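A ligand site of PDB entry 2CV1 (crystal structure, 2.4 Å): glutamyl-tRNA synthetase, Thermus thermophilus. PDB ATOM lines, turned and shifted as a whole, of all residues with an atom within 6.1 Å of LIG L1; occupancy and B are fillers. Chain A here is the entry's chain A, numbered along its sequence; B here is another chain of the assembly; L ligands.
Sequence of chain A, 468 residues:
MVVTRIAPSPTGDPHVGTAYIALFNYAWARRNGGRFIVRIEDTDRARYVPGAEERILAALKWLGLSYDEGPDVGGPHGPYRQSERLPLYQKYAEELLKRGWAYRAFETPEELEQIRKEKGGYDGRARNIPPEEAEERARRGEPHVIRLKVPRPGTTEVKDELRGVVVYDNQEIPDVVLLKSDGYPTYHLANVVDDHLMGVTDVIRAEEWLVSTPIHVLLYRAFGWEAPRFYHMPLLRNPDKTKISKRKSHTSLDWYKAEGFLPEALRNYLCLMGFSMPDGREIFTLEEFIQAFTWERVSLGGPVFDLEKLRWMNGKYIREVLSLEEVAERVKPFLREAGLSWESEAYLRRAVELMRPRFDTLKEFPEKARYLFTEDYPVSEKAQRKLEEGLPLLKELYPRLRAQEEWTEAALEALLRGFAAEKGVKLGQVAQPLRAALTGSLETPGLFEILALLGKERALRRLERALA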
ATOM      1  N   ARG A   5       2.949 -28.949  26.580  1.00  0.00           N
ATOM      2  CA  ARG A   5       2.297 -28.040  27.502  1.00  0.00           C
ATOM      3  C   ARG A   5       1.980 -26.674  26.970  1.00  0.00           C
ATOM      4  O   ARG A   5       2.496 -26.236  25.959  1.00  0.00           O
ATOM      5  CB  ARG A   5       3.098 -27.850  28.791  1.00  0.00           C
ATOM      6  CG  ARG A   5       4.594 -27.500  28.673  1.00  0.00           C
ATOM      7  CD  ARG A   5       4.915 -26.526  27.579  1.00  0.00           C
ATOM      8  NE  ARG A   5       6.248 -25.960  27.687  1.00  0.00           N
ATOM      9  CZ  ARG A   5       6.623 -24.865  27.025  1.00  0.00           C
ATOM     10  NH1 ARG A   5       5.757 -24.278  26.230  1.00  0.00           N
ATOM     11  NH2 ARG A   5       7.813 -24.323  27.214  1.00  0.00           N
ATOM     12  N   ALA A   7       1.768 -22.833  28.662  1.00  0.00           N
ATOM     13  CA  ALA A   7       2.216 -22.157  29.872  1.00  0.00           C
ATOM     14  C   ALA A   7       1.814 -20.682  29.875  1.00  0.00           C
ATOM     15  O   ALA A   7       2.663 -19.787  29.798  1.00  0.00           O
ATOM     16  CB  ALA A   7       3.730 -22.292  29.986  1.00  0.00           C
ATOM     17  N   PRO A   8       0.502 -20.422  29.969  1.00  0.00           N
ATOM     18  CA  PRO A   8      -0.131 -19.096  29.979  1.00  0.00           C
ATOM     19  C   PRO A   8       0.337 -18.242  31.151  1.00  0.00           C
ATOM     20  O   PRO A   8       0.538 -18.755  32.259  1.00  0.00           O
ATOM     21  CB  PRO A   8      -1.630 -19.405  30.104  1.00  0.00           C
ATOM     22  CG  PRO A   8      -1.754 -20.875  29.872  1.00  0.00           C
ATOM     23  CD  PRO A   8      -0.461 -21.466  30.335  1.00  0.00           C
ATOM     24  N   SER A   9       0.510 -16.947  30.894  1.00  0.00           N
ATOM     25  CA  SER A   9       0.914 -15.972  31.930  1.00  0.00           C
ATOM     26  C   SER A   9      -0.403 -15.284  32.266  1.00  0.00           C
ATOM     27  O   SER A   9      -1.057 -14.754  31.376  1.00  0.00           O
ATOM     28  CB  SER A   9       1.928 -14.983  31.352  1.00  0.00           C
ATOM     29  OG  SER A   9       2.506 -14.171  32.353  1.00  0.00           O
ATOM     30  N   ILE A  21      -2.017 -21.796  20.183  1.00  0.00           N
ATOM     31  CA  ILE A  21      -0.857 -22.594  20.553  1.00  0.00           C
ATOM     32  C   ILE A  21      -1.249 -23.839  21.368  1.00  0.00           C
ATOM     33  O   ILE A  21      -0.682 -24.915  21.191  1.00  0.00           O
ATOM     34  CB  ILE A  21       0.160 -21.728  21.337  1.00  0.00           C
ATOM     35  CG1 ILE A  21       0.766 -20.664  20.395  1.00  0.00           C
ATOM     36  CG2 ILE A  21       1.287 -22.603  21.903  1.00  0.00           C
ATOM     37  CD1 ILE A  21       1.580 -21.238  19.250  1.00  0.00           C
ATOM     38  N   ARG A  39       0.585 -25.285  32.766  1.00  0.00           N
ATOM     39  CA  ARG A  39       1.422 -24.710  33.828  1.00  0.00           C
ATOM     40  C   ARG A  39       1.162 -23.217  33.813  1.00  0.00           C
ATOM     41  O   ARG A  39       1.198 -22.601  32.745  1.00  0.00           O
ATOM     42  CB  ARG A  39       2.904 -24.972  33.570  1.00  0.00           C
ATOM     43  CG  ARG A  39       3.839 -24.308  34.615  1.00  0.00           C
ATOM     44  CD  ARG A  39       5.315 -24.719  34.514  1.00  0.00           C
ATOM     45  NE  ARG A  39       5.979 -24.278  33.277  1.00  0.00           N
ATOM     46  CZ  ARG A  39       6.515 -25.104  32.385  1.00  0.00           C
ATOM     47  NH1 ARG A  39       6.471 -26.424  32.571  1.00  0.00           N
ATOM     48  NH2 ARG A  39       7.087 -24.612  31.293  1.00  0.00           N
ATOM     49  N   GLU A  41       2.258 -19.576  34.434  1.00  0.00           N
ATOM     50  CA  GLU A  41       3.509 -18.832  34.491  1.00  0.00           C
ATOM     51  C   GLU A  41       3.310 -17.435  35.096  1.00  0.00           C
ATOM     52  O   GLU A  41       3.340 -16.432  34.400  1.00  0.00           O
ATOM     53  CB  GLU A  41       4.036 -18.795  33.059  1.00  0.00           C
ATOM     54  CG  GLU A  41       5.500 -19.049  32.920  1.00  0.00           C
ATOM     55  CD  GLU A  41       5.880 -20.197  32.010  1.00  0.00           C
ATOM     56  OE1 GLU A  41       5.593 -21.366  32.347  1.00  0.00           O
ATOM     57  OE2 GLU A  41       6.499 -19.923  30.950  1.00  0.00           O
ATOM     58  N   GLN A  82       3.730 -21.397  38.881  1.00  0.00           N
ATOM     59  CA  GLN A  82       5.113 -21.094  39.236  1.00  0.00           C
ATOM     60  C   GLN A  82       5.321 -20.311  40.527  1.00  0.00           C
ATOM     61  O   GLN A  82       6.339 -20.514  41.220  1.00  0.00           O
ATOM     62  CB  GLN A  82       5.806 -20.418  38.055  1.00  0.00           C
ATOM     63  CG  GLN A  82       5.677 -21.220  36.781  1.00  0.00           C
ATOM     64  CD  GLN A  82       6.614 -20.747  35.707  1.00  0.00           C
ATOM     65  OE1 GLN A  82       6.632 -19.557  35.384  1.00  0.00           O
ATOM     66  NE2 GLN A  82       7.393 -21.662  35.134  1.00  0.00           N
ATOM     67  N   TYR A 187      11.281 -15.740  33.226  1.00  0.00           N
ATOM     68  CA  TYR A 187      10.735 -16.698  32.299  1.00  0.00           C
ATOM     69  C   TYR A 187      11.795 -17.731  31.903  1.00  0.00           C
ATOM     70  O   TYR A 187      11.521 -18.944  31.888  1.00  0.00           O
ATOM     71  CB  TYR A 187      10.208 -15.974  31.046  1.00  0.00           C
ATOM     72  CG  TYR A 187      10.031 -16.900  29.860  1.00  0.00           C
ATOM     73  CD1 TYR A 187       8.964 -17.814  29.802  1.00  0.00           C
ATOM     74  CD2 TYR A 187      11.011 -16.964  28.850  1.00  0.00           C
ATOM     75  CE1 TYR A 187       8.888 -18.769  28.789  1.00  0.00           C
ATOM     76  CE2 TYR A 187      10.948 -17.899  27.829  1.00  0.00           C
ATOM     77  CZ  TYR A 187       9.890 -18.811  27.806  1.00  0.00           C
ATOM     78  OH  TYR A 187       9.856 -19.793  26.830  1.00  0.00           O
ATOM     79  N   ASN A 191      11.082 -21.701  33.008  1.00  0.00           N
ATOM     80  CA  ASN A 191      10.615 -22.483  31.862  1.00  0.00           C
ATOM     81  C   ASN A 191      11.428 -23.751  31.686  1.00  0.00           C
ATOM     82  O   ASN A 191      10.872 -24.851  31.558  1.00  0.00           O
ATOM     83  CB  ASN A 191      10.683 -21.590  30.616  1.00  0.00           C
ATOM     84  CG  ASN A 191       9.875 -22.123  29.434  1.00  0.00           C
ATOM     85  OD1 ASN A 191      10.439 -22.702  28.501  1.00  0.00           O
ATOM     86  ND2 ASN A 191       8.547 -21.909  29.451  1.00  0.00           N
ATOM     87  N   ASP A 195      10.001 -27.325  32.693  1.00  0.00           N
ATOM     88  CA  ASP A 195       9.787 -28.256  31.589  1.00  0.00           C
ATOM     89  C   ASP A 195      10.524 -29.571  31.867  1.00  0.00           C
ATOM     90  O   ASP A 195      10.022 -30.663  31.577  1.00  0.00           O
ATOM     91  CB  ASP A 195      10.278 -27.669  30.263  1.00  0.00           C
ATOM     92  CG  ASP A 195       9.251 -26.751  29.612  1.00  0.00           C
ATOM     93  OD1 ASP A 195       9.648 -26.048  28.658  1.00  0.00           O
ATOM     94  OD2 ASP A 195       8.069 -26.737  30.062  1.00  0.00           O
ATOM     95  N   VAL A 203       8.329 -29.042  23.045  1.00  0.00           N
ATOM     96  CA  VAL A 203       7.934 -27.663  23.258  1.00  0.00           C
ATOM     97  C   VAL A 203       7.419 -27.064  21.944  1.00  0.00           C
ATOM     98  O   VAL A 203       8.159 -26.884  20.974  1.00  0.00           O
ATOM     99  CB  VAL A 203       9.115 -26.844  23.804  1.00  0.00           C
ATOM    100  CG1 VAL A 203       8.739 -25.349  23.952  1.00  0.00           C
ATOM    101  CG2 VAL A 203       9.539 -27.422  25.139  1.00  0.00           C
ATOM    102  N   ILE A 204       6.126 -26.792  21.916  1.00  0.00           N
ATOM    103  CA  ILE A 204       5.488 -26.182  20.751  1.00  0.00           C
ATOM    104  C   ILE A 204       5.052 -24.813  21.246  1.00  0.00           C
ATOM    105  O   ILE A 204       4.259 -24.705  22.168  1.00  0.00           O
ATOM    106  CB  ILE A 204       4.259 -26.983  20.314  1.00  0.00           C
ATOM    107  CG1 ILE A 204       4.664 -28.442  20.111  1.00  0.00           C
ATOM    108  CG2 ILE A 204       3.672 -26.389  19.061  1.00  0.00           C
ATOM    109  CD1 ILE A 204       3.505 -29.386  20.045  1.00  0.00           C
ATOM    110  N   ARG A 205       5.550 -23.755  20.629  1.00  0.00           N
ATOM    111  CA  ARG A 205       5.221 -22.418  21.088  1.00  0.00           C
ATOM    112  C   ARG A 205       5.346 -21.439  19.918  1.00  0.00           C
ATOM    113  O   ARG A 205       5.889 -21.775  18.877  1.00  0.00           O
ATOM    114  CB  ARG A 205       6.184 -22.048  22.228  1.00  0.00           C
ATOM    115  CG  ARG A 205       7.428 -21.344  21.736  1.00  0.00           C
ATOM    116  CD  ARG A 205       8.758 -21.991  22.121  1.00  0.00           C
ATOM    117  NE  ARG A 205       9.053 -21.970  23.549  1.00  0.00           N
ATOM    118  CZ  ARG A 205      10.280 -22.015  24.078  1.00  0.00           C
ATOM    119  NH1 ARG A 205      11.374 -22.061  23.326  1.00  0.00           N
ATOM    120  NH2 ARG A 205      10.413 -22.082  25.395  1.00  0.00           N
ATOM    121  N   ALA A 206       4.827 -20.232  20.102  1.00  0.00           N
ATOM    122  CA  ALA A 206       4.860 -19.224  19.047  1.00  0.00           C
ATOM    123  C   ALA A 206       6.268 -18.780  18.714  1.00  0.00           C
ATOM    124  O   ALA A 206       7.151 -18.641  19.569  1.00  0.00           O
ATOM    125  CB  ALA A 206       4.028 -18.021  19.444  1.00  0.00           C
ATOM    126  N   GLU A 208       7.538 -16.143  18.335  1.00  0.00           N
ATOM    127  CA  GLU A 208       8.110 -15.031  19.047  1.00  0.00           C
ATOM    128  C   GLU A 208       9.210 -15.465  20.016  1.00  0.00           C
ATOM    129  O   GLU A 208      10.041 -14.636  20.413  1.00  0.00           O
ATOM    130  CB  GLU A 208       7.037 -14.224  19.783  1.00  0.00           C
ATOM    131  CG  GLU A 208       6.480 -14.886  21.029  1.00  0.00           C
ATOM    132  CD  GLU A 208       5.518 -13.966  21.804  1.00  0.00           C
ATOM    133  OE1 GLU A 208       5.978 -13.007  22.481  1.00  0.00           O
ATOM    134  OE2 GLU A 208       4.299 -14.209  21.743  1.00  0.00           O
ATOM    135  N   TRP A 209       9.255 -16.763  20.378  1.00  0.00           N
ATOM    136  CA  TRP A 209      10.247 -17.269  21.327  1.00  0.00           C
ATOM    137  C   TRP A 209      11.473 -17.938  20.695  1.00  0.00           C
ATOM    138  O   TRP A 209      12.383 -18.380  21.411  1.00  0.00           O
ATOM    139  CB  TRP A 209       9.604 -18.282  22.284  1.00  0.00           C
ATOM    140  CG  TRP A 209       8.372 -17.811  22.948  1.00  0.00           C
ATOM    141  CD1 TRP A 209       7.094 -18.066  22.562  1.00  0.00           C
ATOM    142  CD2 TRP A 209       8.276 -16.966  24.102  1.00  0.00           C
ATOM    143  NE1 TRP A 209       6.207 -17.434  23.383  1.00  0.00           N
ATOM    144  CE2 TRP A 209       6.895 -16.756  24.345  1.00  0.00           C
ATOM    145  CE3 TRP A 209       9.214 -16.376  24.954  1.00  0.00           C
ATOM    146  CZ2 TRP A 209       6.432 -15.968  25.402  1.00  0.00           C
ATOM    147  CZ3 TRP A 209       8.761 -15.588  26.014  1.00  0.00           C
ATOM    148  CH2 TRP A 209       7.376 -15.389  26.235  1.00  0.00           C
ATOM    149  N   HIS A 216      17.797 -21.018  26.322  1.00  0.00           N
ATOM    150  CA  HIS A 216      17.276 -22.248  26.924  1.00  0.00           C
ATOM    151  C   HIS A 216      18.156 -23.458  26.702  1.00  0.00           C
ATOM    152  O   HIS A 216      18.331 -24.287  27.592  1.00  0.00           O
ATOM    153  CB  HIS A 216      15.874 -22.473  26.399  1.00  0.00           C
ATOM    154  CG  HIS A 216      14.969 -21.336  26.702  1.00  0.00           C
ATOM    155  ND1 HIS A 216      13.736 -21.195  26.122  1.00  0.00           N
ATOM    156  CD2 HIS A 216      15.146 -20.247  27.496  1.00  0.00           C
ATOM    157  CE1 HIS A 216      13.185 -20.061  26.533  1.00  0.00           C
ATOM    158  NE2 HIS A 216      14.034 -19.462  27.365  1.00  0.00           N
ATOM    159  P     A B  75       8.892 -12.427  33.797  1.00  0.00           P
ATOM    160  OP1   A B  75       9.116 -12.910  35.185  1.00  0.00           O
ATOM    161  OP2   A B  75       9.820 -12.857  32.711  1.00  0.00           O
ATOM    162  O5'   A B  75       7.395 -12.832  33.411  1.00  0.00           O
ATOM    163  C5'   A B  75       7.101 -14.094  32.855  1.00  0.00           C
ATOM    164  C4'   A B  75       6.067 -13.959  31.771  1.00  0.00           C
ATOM    165  O4'   A B  75       6.274 -12.729  31.033  1.00  0.00           O
ATOM    166  C3'   A B  75       6.190 -15.083  30.773  1.00  0.00           C
ATOM    167  O3'   A B  75       5.590 -16.245  31.322  1.00  0.00           O
ATOM    168  C2'   A B  75       5.723 -14.423  29.471  1.00  0.00           C
ATOM    169  O2'   A B  75       4.331 -14.423  29.282  1.00  0.00           O
ATOM    170  C1'   A B  75       6.248 -12.998  29.638  1.00  0.00           C
ATOM    171  N9    A B  75       7.604 -12.817  29.127  1.00  0.00           N
ATOM    172  C8    A B  75       8.771 -12.959  29.843  1.00  0.00           C
ATOM    173  N7    A B  75       9.850 -12.792  29.124  1.00  0.00           N
ATOM    174  C5    A B  75       9.372 -12.531  27.847  1.00  0.00           C
ATOM    175  C6    A B  75      10.017 -12.309  26.619  1.00  0.00           C
ATOM    176  N6    A B  75      11.351 -12.362  26.476  1.00  0.00           N
ATOM    177  N1    A B  75       9.255 -12.064  25.534  1.00  0.00           N
ATOM    178  C2    A B  75       7.917 -12.060  25.690  1.00  0.00           C
ATOM    179  N3    A B  75       7.190 -12.281  26.784  1.00  0.00           N
ATOM    180  C4    A B  75       7.981 -12.518  27.847  1.00  0.00           C
HETATM  181  N1  LIG L   1       4.931 -18.232  29.882  1.00  0.00           N
HETATM  182  C1  LIG L   1       5.082 -18.234  28.443  1.00  0.00           C
HETATM  183  C2  LIG L   1       5.506 -19.633  27.956  1.00  0.00           C
HETATM  184  C3  LIG L   1       5.913 -19.709  26.481  1.00  0.00           C
HETATM  185  C4  LIG L   1       6.609 -21.020  26.120  1.00  0.00           C
HETATM  186  O1  LIG L   1       5.927 -21.872  25.532  1.00  0.00           O
HETATM  187  O2  LIG L   1       7.813 -21.202  26.408  1.00  0.00           O
HETATM  188  C5  LIG L   1       3.760 -17.847  27.795  1.00  0.00           C
HETATM  189  O3  LIG L   1       3.982 -17.286  26.519  1.00  0.00           O
HETATM  190  P1  LG2 L   2       2.264 -12.020  27.923  1.00  0.00           P
HETATM  191  O1  LG2 L   2       3.567 -12.187  27.154  1.00  0.00           O
HETATM  192  O2  LG2 L   2       1.704 -10.615  27.645  1.00  0.00           O
HETATM  193  O3  LG2 L   2       2.496 -12.124  29.423  1.00  0.00           O
HETATM  194  P2  LG2 L   2       1.045 -13.921  25.973  1.00  0.00           P
HETATM  195  O4  LG2 L   2       2.423 -14.278  25.497  1.00  0.00           O
HETATM  196  O5  LG2 L   2       0.309 -13.131  24.931  1.00  0.00           O
HETATM  197  O6  LG2 L   2       1.070 -13.057  27.398  1.00  0.00           O
HETATM  198  P3  LG2 L   2       0.475 -16.351  27.437  1.00  0.00           P
HETATM  199  O7  LG2 L   2       1.542 -15.955  28.388  1.00  0.00           O
HETATM  200  O8  LG2 L   2      -0.778 -16.749  28.157  1.00  0.00           O
HETATM  201  O9  LG2 L   2       0.132 -15.197  26.331  1.00  0.00           O
HETATM  202  O10 LG2 L   2       1.022 -17.540  26.532  1.00  0.00           O
HETATM  203  C1  LG2 L   2       0.132 -18.080  25.535  1.00  0.00           C
HETATM  204  C2  LG2 L   2       0.762 -19.081  24.591  1.00  0.00           C
HETATM  205  O11 LG2 L   2       0.373 -18.716  23.231  1.00  0.00           O
HETATM  206  C3  LG2 L   2       2.317 -19.180  24.515  1.00  0.00           C
HETATM  207  O12 LG2 L   2       2.782 -20.526  24.217  1.00  0.00           O
HETATM  208  C4  LG2 L   2       2.673 -18.133  23.470  1.00  0.00           C
HETATM  209  O13 LG2 L   2       3.858 -18.467  22.748  1.00  0.00           O
HETATM  210  C5  LG2 L   2       1.474 -18.138  22.510  1.00  0.00           C
HETATM  211  N1  LG2 L   2       1.075 -16.790  22.005  1.00  0.00           N
HETATM  212  C6  LG2 L   2       0.936 -15.598  22.697  1.00  0.00           C
HETATM  213  N2  LG2 L   2       0.561 -14.587  21.950  1.00  0.00           N
HETATM  214  C7  LG2 L   2       0.436 -15.129  20.680  1.00  0.00           C
HETATM  215  C8  LG2 L   2       0.073 -14.566  19.419  1.00  0.00           C
HETATM  216  N3  LG2 L   2      -0.247 -13.272  19.283  1.00  0.00           N
HETATM  217  N4  LG2 L   2       0.045 -15.397  18.318  1.00  0.00           N
HETATM  218  C9  LG2 L   2       0.371 -16.710  18.468  1.00  0.00           C
HETATM  219  N5  LG2 L   2       0.731 -17.341  19.616  1.00  0.00           N
HETATM  220  C10 LG2 L   2       0.746 -16.492  20.691  1.00  0.00           C
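O3 of LIG L1 lies within hydrogen-bond range of O10 of LG2 L2.
OD1 of Asn 191 is in hydrogen-bond range of NH2 of Arg 5 (3.3 Å). The guanidinium group (NH2) of Arg 205 lies within hydrogen-bond range of the side-chain hydroxyl (OH) of Tyr 187 (2.8 Å). The backbone NH (N) of Glu 41 is in hydrogen-bond range of the backbone carbonyl oxygen (O) of Pro 8 (2.9 Å). The backbone NH of Tyr 187 is in hydrogen-bond range of OP2 of A 75 of chain B. OD1 of Asn 191 lies close to OD1 of Asp 195 (3.4 Å). OH of Tyr 187 lies within hydrogen-bond range of OD1 of Asn 191 (3.4 Å). OE1 of Glu 41 lies within hydrogen-bond range of NE2 of Gln 82, at 3.3 Å. The guanidinium group (NH2) of Arg 5 is in salt-bridge range of the side-chain carboxylate (OD1) of Asp 195 (2.9 Å).
Trp 209 touches LIG L1. Hydrophobic or aromatic side chains that line LIG L1: Ala 7, Tyr 187 and Trp 209. Eight residues have an atom within 4 Å of LIG L1: Arg 5, Ala 7, Glu 41, Tyr 187, Asn 191, Arg 205, Trp 209 and A 75 of chain B.
O13 of LG2 L2 lies within hydrogen-bond range of NE1 of Trp 209, 2.6 Å away. O1 of LIG L1 lies within salt-bridge range of NH1 of Arg 5. O13 of LG2 L2 lies within hydrogen-bond range of N of Ala 206, 3.3 Å away. A nitrogen (N1) of LIG L1 is in hydrogen-bond range of the backbone carbonyl oxygen (O) of Ala 7 (2.8 Å). The side-chain carboxylate (OE2) of Glu 41 lies within salt-bridge range of a nitrogen (N1) of LIG L1 (2.5 Å). The side-chain hydroxyl of Tyr 187 sits at hydrogen-bond distance from an oxygen (O2) of LIG L1. O2 of LIG L1 lies within hydrogen-bond range of ND2 of Asn 191 (3.2 Å). O2' of A 75 of chain B lies close to O3 of LG2 L2, 2.9 Å away. O3' of A 75 of chain B sits at hydrogen-bond distance from a nitrogen (N1) of LIG L1. The guanidinium group of Arg 205 lies within salt-bridge range of an oxygen (O2) of LIG L1. N of Ser 9 lies within hydrogen-bond range of O7 of LG2 L2.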
